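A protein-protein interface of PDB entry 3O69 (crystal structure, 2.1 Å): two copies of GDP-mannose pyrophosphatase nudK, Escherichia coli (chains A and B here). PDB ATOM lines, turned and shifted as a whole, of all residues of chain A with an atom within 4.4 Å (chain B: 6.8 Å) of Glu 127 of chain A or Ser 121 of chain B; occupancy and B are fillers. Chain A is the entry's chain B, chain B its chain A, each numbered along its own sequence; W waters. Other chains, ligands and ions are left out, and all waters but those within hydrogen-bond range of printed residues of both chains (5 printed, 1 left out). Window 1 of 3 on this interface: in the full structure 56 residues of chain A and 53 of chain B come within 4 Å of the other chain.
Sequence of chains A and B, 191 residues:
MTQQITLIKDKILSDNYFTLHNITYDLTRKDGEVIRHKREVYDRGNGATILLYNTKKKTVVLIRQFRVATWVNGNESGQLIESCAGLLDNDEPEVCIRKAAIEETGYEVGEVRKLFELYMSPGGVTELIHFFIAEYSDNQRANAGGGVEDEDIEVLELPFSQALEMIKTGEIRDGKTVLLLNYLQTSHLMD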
ATOM      1  N   ARG A  44      14.947  -1.908   1.173  1.00  0.00           N
ATOM      2  CA  ARG A  44      14.082  -2.790   1.944  1.00  0.00           C
ATOM      3  C   ARG A  44      13.374  -2.044   3.070  1.00  0.00           C
ATOM      4  O   ARG A  44      12.690  -2.663   3.898  1.00  0.00           O
ATOM      5  CB  ARG A  44      14.891  -3.928   2.559  1.00  0.00           C
ATOM      6  CG  ARG A  44      15.386  -4.962   1.584  1.00  0.00           C
ATOM      7  CD  ARG A  44      16.137  -6.055   2.325  1.00  0.00           C
ATOM      8  NE  ARG A  44      15.219  -7.016   2.926  1.00  0.00           N
ATOM      9  CZ  ARG A  44      14.910  -7.079   4.219  1.00  0.00           C
ATOM     10  NH1 ARG A  44      15.443  -6.233   5.117  1.00  0.00           N
ATOM     11  NH2 ARG A  44      14.058  -8.004   4.615  1.00  0.00           N
ATOM     12  N   GLY A  45      13.551  -0.723   3.104  1.00  0.00           N
ATOM     13  CA  GLY A  45      13.035   0.108   4.194  1.00  0.00           C
ATOM     14  C   GLY A  45      13.913   0.057   5.448  1.00  0.00           C
ATOM     15  O   GLY A  45      14.917  -0.653   5.504  1.00  0.00           O
ATOM     16  N   ASN A  46      13.523   0.823   6.456  1.00  0.00           N
ATOM     17  CA  ASN A  46      14.272   0.919   7.698  1.00  0.00           C
ATOM     18  C   ASN A  46      13.700  -0.037   8.754  1.00  0.00           C
ATOM     19  O   ASN A  46      12.580  -0.562   8.598  1.00  0.00           O
ATOM     20  CB  ASN A  46      14.297   2.381   8.197  1.00  0.00           C
ATOM     21  CG  ASN A  46      15.057   3.322   7.251  1.00  0.00           C
ATOM     22  OD1 ASN A  46      15.899   2.895   6.469  1.00  0.00           O
ATOM     23  ND2 ASN A  46      14.773   4.611   7.348  1.00  0.00           N
ATOM     24  N   LEU A 118      21.796   4.025  12.582  1.00  0.00           N
ATOM     25  CA  LEU A 118      22.939   3.733  11.739  1.00  0.00           C
ATOM     26  C   LEU A 118      22.537   3.134  10.408  1.00  0.00           C
ATOM     27  O   LEU A 118      21.681   2.255  10.350  1.00  0.00           O
ATOM     28  CB  LEU A 118      23.876   2.751  12.459  1.00  0.00           C
ATOM     29  CG  LEU A 118      24.279   3.083  13.909  1.00  0.00           C
ATOM     30  CD1 LEU A 118      25.241   2.031  14.454  1.00  0.00           C
ATOM     31  CD2 LEU A 118      24.880   4.487  14.017  1.00  0.00           C
ATOM     32  N   TYR A 119      23.179   3.614   9.354  1.00  0.00           N
ATOM     33  CA  TYR A 119      23.173   2.959   8.063  1.00  0.00           C
ATOM     34  C   TYR A 119      24.099   1.751   8.205  1.00  0.00           C
ATOM     35  O   TYR A 119      25.259   1.901   8.589  1.00  0.00           O
ATOM     36  CB  TYR A 119      23.681   3.923   6.964  1.00  0.00           C
ATOM     37  CG  TYR A 119      22.766   5.104   6.681  1.00  0.00           C
ATOM     38  CD1 TYR A 119      21.513   4.906   6.101  1.00  0.00           C
ATOM     39  CD2 TYR A 119      23.156   6.422   6.995  1.00  0.00           C
ATOM     40  CE1 TYR A 119      20.656   5.984   5.838  1.00  0.00           C
ATOM     41  CE2 TYR A 119      22.320   7.504   6.728  1.00  0.00           C
ATOM     42  CZ  TYR A 119      21.072   7.274   6.151  1.00  0.00           C
ATOM     43  OH  TYR A 119      20.227   8.318   5.879  1.00  0.00           O
ATOM     44  N   MET A 120      23.559   0.565   7.923  1.00  0.00           N
ATOM     45  CA  MET A 120      24.253  -0.710   8.099  1.00  0.00           C
ATOM     46  C   MET A 120      25.026  -1.226   6.890  1.00  0.00           C
ATOM     47  O   MET A 120      26.001  -1.939   7.056  1.00  0.00           O
ATOM     48  CB  MET A 120      23.261  -1.778   8.556  1.00  0.00           C
ATOM     49  CG  MET A 120      22.695  -1.524   9.947  1.00  0.00           C
ATOM     50  SD  MET A 120      23.987  -1.364  11.205  1.00  0.00           S
ATOM     51  CE  MET A 120      24.413  -3.106  11.429  1.00  0.00           C
ATOM     52  N   VAL A 125      22.734  -0.465  -0.076  1.00  0.00           N
ATOM     53  CA  VAL A 125      21.540  -0.771   0.705  1.00  0.00           C
ATOM     54  C   VAL A 125      21.160   0.470   1.507  1.00  0.00           C
ATOM     55  O   VAL A 125      21.986   1.132   2.125  1.00  0.00           O
ATOM     56  CB  VAL A 125      21.695  -2.076   1.596  1.00  0.00           C
ATOM     57  CG1 VAL A 125      20.340  -2.560   2.156  1.00  0.00           C
ATOM     58  CG2 VAL A 125      22.360  -3.211   0.799  1.00  0.00           C
ATOM     59  N   THR A 126      19.882   0.778   1.422  1.00  0.00           N
ATOM     60  CA  THR A 126      19.235   1.941   1.985  1.00  0.00           C
ATOM     61  C   THR A 126      19.115   1.843   3.520  1.00  0.00           C
ATOM     62  O   THR A 126      19.178   2.871   4.245  1.00  0.00           O
ATOM     63  CB  THR A 126      17.836   1.967   1.296  1.00  0.00           C
ATOM     64  OG1 THR A 126      17.668   3.125   0.464  1.00  0.00           O
ATOM     65  CG2 THR A 126      16.721   1.736   2.221  1.00  0.00           C
ATOM     66  N   GLU A 127      18.961   0.608   4.006  1.00  0.00           N
ATOM     67  CA  GLU A 127      18.623   0.320   5.407  1.00  0.00           C
ATOM     68  C   GLU A 127      19.259   1.227   6.472  1.00  0.00           C
ATOM     69  O   GLU A 127      20.482   1.248   6.634  1.00  0.00           O
ATOM     70  CB  GLU A 127      18.944  -1.147   5.729  1.00  0.00           C
ATOM     71  CG  GLU A 127      18.525  -1.597   7.129  1.00  0.00           C
ATOM     72  CD  GLU A 127      18.908  -3.030   7.402  1.00  0.00           C
ATOM     73  OE1 GLU A 127      20.119  -3.322   7.508  1.00  0.00           O
ATOM     74  OE2 GLU A 127      18.001  -3.874   7.490  1.00  0.00           O
ATOM     75  N   LEU A 128      18.423   1.940   7.213  1.00  0.00           N
ATOM     76  CA  LEU A 128      18.848   2.593   8.463  1.00  0.00           C
ATOM     77  C   LEU A 128      18.237   1.826   9.648  1.00  0.00           C
ATOM     78  O   LEU A 128      17.056   1.493   9.626  1.00  0.00           O
ATOM     79  CB  LEU A 128      18.423   4.065   8.469  1.00  0.00           C
ATOM     80  CG  LEU A 128      18.738   4.940   9.684  1.00  0.00           C
ATOM     81  CD1 LEU A 128      19.970   5.813   9.452  1.00  0.00           C
ATOM     82  CD2 LEU A 128      17.534   5.820   9.998  1.00  0.00           C
ATOM     83  N   ILE A 129      19.054   1.520  10.661  1.00  0.00           N
ATOM     84  CA  ILE A 129      18.583   0.798  11.861  1.00  0.00           C
ATOM     85  C   ILE A 129      18.615   1.705  13.117  1.00  0.00           C
ATOM     86  O   ILE A 129      19.634   2.322  13.415  1.00  0.00           O
ATOM     87  CB  ILE A 129      19.382  -0.501  12.111  1.00  0.00           C
ATOM     88  CG1 ILE A 129      19.282  -1.471  10.913  1.00  0.00           C
ATOM     89  CG2 ILE A 129      18.956  -1.183  13.438  1.00  0.00           C
ATOM     90  CD1 ILE A 129      17.917  -2.090  10.710  1.00  0.00           C
ATOM     91  N   ALA B  69      22.812   5.480  -1.699  1.00  0.00           N
ATOM     92  CA  ALA B  69      21.817   4.697  -0.974  1.00  0.00           C
ATOM     93  C   ALA B  69      21.387   5.410   0.311  1.00  0.00           C
ATOM     94  O   ALA B  69      20.256   5.245   0.774  1.00  0.00           O
ATOM     95  CB  ALA B  69      22.350   3.289  -0.681  1.00  0.00           C
ATOM     96  N   ASN B  73      17.651   7.986   1.158  1.00  0.00           N
ATOM     97  CA  ASN B  73      17.026   7.567   2.417  1.00  0.00           C
ATOM     98  C   ASN B  73      17.406   8.464   3.618  1.00  0.00           C
ATOM     99  O   ASN B  73      17.972   7.985   4.602  1.00  0.00           O
ATOM    100  CB  ASN B  73      17.330   6.078   2.716  1.00  0.00           C
ATOM    101  CG  ASN B  73      16.566   5.546   3.937  1.00  0.00           C
ATOM    102  OD1 ASN B  73      15.467   6.013   4.239  1.00  0.00           O
ATOM    103  ND2 ASN B  73      17.147   4.549   4.633  1.00  0.00           N
ATOM    104  N   LEU B 118      31.315 -10.270  10.196  1.00  0.00           N
ATOM    105  CA  LEU B 118      29.914 -10.077  10.572  1.00  0.00           C
ATOM    106  C   LEU B 118      28.977  -9.831   9.395  1.00  0.00           C
ATOM    107  O   LEU B 118      29.294  -9.049   8.501  1.00  0.00           O
ATOM    108  CB  LEU B 118      29.782  -8.898  11.556  1.00  0.00           C
ATOM    109  CG  LEU B 118      30.683  -8.850  12.791  1.00  0.00           C
ATOM    110  CD1 LEU B 118      30.458  -7.555  13.536  1.00  0.00           C
ATOM    111  CD2 LEU B 118      30.423 -10.062  13.696  1.00  0.00           C
ATOM    112  N   TYR B 119      27.813 -10.491   9.418  1.00  0.00           N
ATOM    113  CA  TYR B 119      26.742 -10.219   8.447  1.00  0.00           C
ATOM    114  C   TYR B 119      26.102  -8.929   8.885  1.00  0.00           C
ATOM    115  O   TYR B 119      25.761  -8.784  10.052  1.00  0.00           O
ATOM    116  CB  TYR B 119      25.682 -11.329   8.429  1.00  0.00           C
ATOM    117  CG  TYR B 119      26.203 -12.667   7.981  1.00  0.00           C
ATOM    118  CD1 TYR B 119      26.527 -12.903   6.642  1.00  0.00           C
ATOM    119  CD2 TYR B 119      26.387 -13.700   8.896  1.00  0.00           C
ATOM    120  CE1 TYR B 119      27.028 -14.150   6.230  1.00  0.00           C
ATOM    121  CE2 TYR B 119      26.873 -14.941   8.492  1.00  0.00           C
ATOM    122  CZ  TYR B 119      27.189 -15.159   7.163  1.00  0.00           C
ATOM    123  OH  TYR B 119      27.673 -16.396   6.782  1.00  0.00           O
ATOM    124  N   MET B 120      25.942  -7.989   7.957  1.00  0.00           N
ATOM    125  CA  MET B 120      25.586  -6.619   8.338  1.00  0.00           C
ATOM    126  C   MET B 120      24.103  -6.330   8.200  1.00  0.00           C
ATOM    127  O   MET B 120      23.562  -5.470   8.892  1.00  0.00           O
ATOM    128  CB  MET B 120      26.420  -5.602   7.549  1.00  0.00           C
ATOM    129  CG  MET B 120      27.883  -5.524   8.003  1.00  0.00           C
ATOM    130  SD  MET B 120      28.073  -5.188   9.761  1.00  0.00           S
ATOM    131  CE  MET B 120      27.744  -3.424   9.862  1.00  0.00           C
ATOM    132  N   SER B 121      23.455  -7.039   7.285  1.00  0.00           N
ATOM    133  CA  SER B 121      22.032  -6.822   7.020  1.00  0.00           C
ATOM    134  C   SER B 121      21.361  -8.132   6.592  1.00  0.00           C
ATOM    135  O   SER B 121      20.932  -8.264   5.449  1.00  0.00           O
ATOM    136  CB  SER B 121      21.866  -5.730   5.963  1.00  0.00           C
ATOM    137  OG  SER B 121      20.502  -5.389   5.829  1.00  0.00           O
ATOM    138  N   PRO B 122      21.262  -9.104   7.526  1.00  0.00           N
ATOM    139  CA  PRO B 122      20.840 -10.487   7.209  1.00  0.00           C
ATOM    140  C   PRO B 122      19.353 -10.701   6.902  1.00  0.00           C
ATOM    141  O   PRO B 122      18.979 -11.785   6.477  1.00  0.00           O
ATOM    142  CB  PRO B 122      21.231 -11.266   8.460  1.00  0.00           C
ATOM    143  CG  PRO B 122      21.127 -10.238   9.579  1.00  0.00           C
ATOM    144  CD  PRO B 122      21.575  -8.936   8.960  1.00  0.00           C
ATOM    145  N   GLY B 123      18.521  -9.681   7.097  1.00  0.00           N
ATOM    146  CA  GLY B 123      17.127  -9.725   6.662  1.00  0.00           C
ATOM    147  C   GLY B 123      16.943 -10.145   5.213  1.00  0.00           C
ATOM    148  O   GLY B 123      16.116 -11.015   4.912  1.00  0.00           O
ATOM    149  N   GLY B 124      17.720  -9.552   4.314  1.00  0.00           N
ATOM    150  CA  GLY B 124      17.574  -9.829   2.884  1.00  0.00           C
ATOM    151  C   GLY B 124      18.805  -9.577   2.022  1.00  0.00           C
ATOM    152  O   GLY B 124      18.698  -9.540   0.786  1.00  0.00           O
ATOM    153  N   VAL B 125      19.965  -9.409   2.673  1.00  0.00           N
ATOM    154  CA  VAL B 125      21.248  -9.140   2.000  1.00  0.00           C
ATOM    155  C   VAL B 125      22.308 -10.130   2.504  1.00  0.00           C
ATOM    156  O   VAL B 125      22.454 -10.318   3.712  1.00  0.00           O
ATOM    157  CB  VAL B 125      21.728  -7.665   2.199  1.00  0.00           C
ATOM    158  CG1 VAL B 125      22.968  -7.368   1.342  1.00  0.00           C
ATOM    159  CG2 VAL B 125      20.617  -6.663   1.840  1.00  0.00           C
ATOM    160  N   THR B 126      23.039 -10.763   1.586  1.00  0.00           N
ATOM    161  CA  THR B 126      24.051 -11.780   1.952  1.00  0.00           C
ATOM    162  C   THR B 126      25.278 -11.224   2.673  1.00  0.00           C
ATOM    163  O   THR B 126      25.955 -11.965   3.394  1.00  0.00           O
ATOM    164  CB  THR B 126      24.551 -12.582   0.721  1.00  0.00           C
ATOM    165  OG1 THR B 126      25.386 -11.761  -0.101  1.00  0.00           O
ATOM    166  CG2 THR B 126      23.399 -13.091  -0.114  1.00  0.00           C
ATOM    167  N   GLU B 127      25.541  -9.927   2.480  1.00  0.00           N
ATOM    168  CA  GLU B 127      26.822  -9.268   2.795  1.00  0.00           C
ATOM    169  C   GLU B 127      27.465  -9.593   4.131  1.00  0.00           C
ATOM    170  O   GLU B 127      26.879  -9.333   5.200  1.00  0.00           O
ATOM    171  CB  GLU B 127      26.692  -7.745   2.690  1.00  0.00           C
ATOM    172  CG  GLU B 127      28.012  -7.007   2.927  1.00  0.00           C
ATOM    173  CD  GLU B 127      27.827  -5.510   2.999  1.00  0.00           C
ATOM    174  OE1 GLU B 127      27.229  -5.027   3.979  1.00  0.00           O
ATOM    175  OE2 GLU B 127      28.289  -4.826   2.068  1.00  0.00           O
HETATM  176  O   HOH W   1      18.022  -6.706   8.092  1.00  0.00           O
HETATM  177  O   HOH W   2      20.998  -4.631   9.750  1.00  0.00           O
HETATM  178  O   HOH W   3      28.105  -3.052   5.674  1.00  0.00           O
HETATM  179  O   HOH W   4      18.239  -6.788   4.748  1.00  0.00           O
HETATM  180  O   HOH W   5      15.560   7.221   6.662  1.00  0.00           O
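O of Ala 69 of chain B sits at hydrogen-bond distance from OG1 of Thr 126 of chain A (3.4 Å).
ND2 of Asn 73 of chain B lies within hydrogen-bond range of OD1 of Asn 46 of chain A, at 2.8 Å.
The side-chain hydroxyl (OH) of Tyr 119 of chain A sits at hydrogen-bond distance from the backbone carbonyl oxygen (O) of Asn 73 of chain B, 2.6 Å away.
The side-chain amide nitrogen (ND2) of Asn 73 of chain B is in hydrogen-bond range of the backbone carbonyl oxygen (O) of Thr 126 of chain A (2.7 Å).
The side-chain hydroxyl (OG) of Ser 121 of chain B sits at hydrogen-bond distance from the side-chain carboxylate (OE1) of Glu 127 of chain A.
O of Glu 127 of chain B is in hydrogen-bond range of N of Met 120 of chain B, 3.2 Å away.
The side-chain amide oxygen (OD1) of Asn 46 of chain A sits at hydrogen-bond distance from the backbone NH (N) of Leu 128 of chain A, at 2.8 Å.
O of Glu 127 of chain A lies within hydrogen-bond range of N of Met 120 of chain A (3.4 Å).
Among the printed residues, pairs that only touch across the chains: Val 125 of chain A with Ala 69 of chain B, Met 120 of chain A with Met 120 of chain B, Arg 44 of chain A with Gly 123 of chain B, Arg 44 of chain A with Gly 124 of chain B and Leu 128 of chain A with Asn 73 of chain B.
Glu 127 of chain A touches just one residue of chain B: Ser 121.
Printed residues of chain A within 4 Å of Ser 121 of chain B: Glu 127.
Printed residues of chain A within 4 Å of Gly 123 of chain B: Arg 44 (3.6 Å).
Of the printed residues of chain A, Ala 69 of chain B touches Val 125 and Thr 126.
Ile 129 of chain A touches none of the printed residues of chain B.
The nearest printed residue of chain B that does not touch Val 125 of chain A is Val 125 of chain B (4.005 Å).
Hydrophobic or aromatic side chains of chain A within 4 Å of the printed part of chain B: Tyr 119 and Met 120.
Among the printed residues, 10 pairs touch across the chains.
Among the printed residues, no Asp or Glu carboxylate lies within 4 Å of a Lys or Arg side-chain nitrogen of the other chain.
Met 120 of chain B touches its own counterpart, Met 120 of chain A.
Positions printed for both chains: 118, 119, 120, 125, 126 and 127.
Of the 10 pairs that touch across the chains among the printed residues, 1 has its exchanged pair printed and touching as well.
Water W5 lies within hydrogen-bond range of OD1 of Asn 73 of chain B and ND2 of Asn 46 of chain A.
Water W2 lies within hydrogen-bond range of OE1 of Glu 127 of chain A and O of Met 120 of chain B.
Water W3 lies within hydrogen-bond range of OE1 of Glu 127 of chain B (2.7 Å) and O of Met 120 of chain A (2.8 Å).
Water W4 lies within hydrogen-bond range of the backbone NH (N) of Gly 124 of chain B, the side-chain hydroxyl (OG) of Ser 121 of chain B and the guanidinium group (NH1) of Arg 44 of chain A.
Water W1 bridges OE2 of Glu 127 of chain A (2.9 Å) and N of Gly 123 of chain B (3.2 Å).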
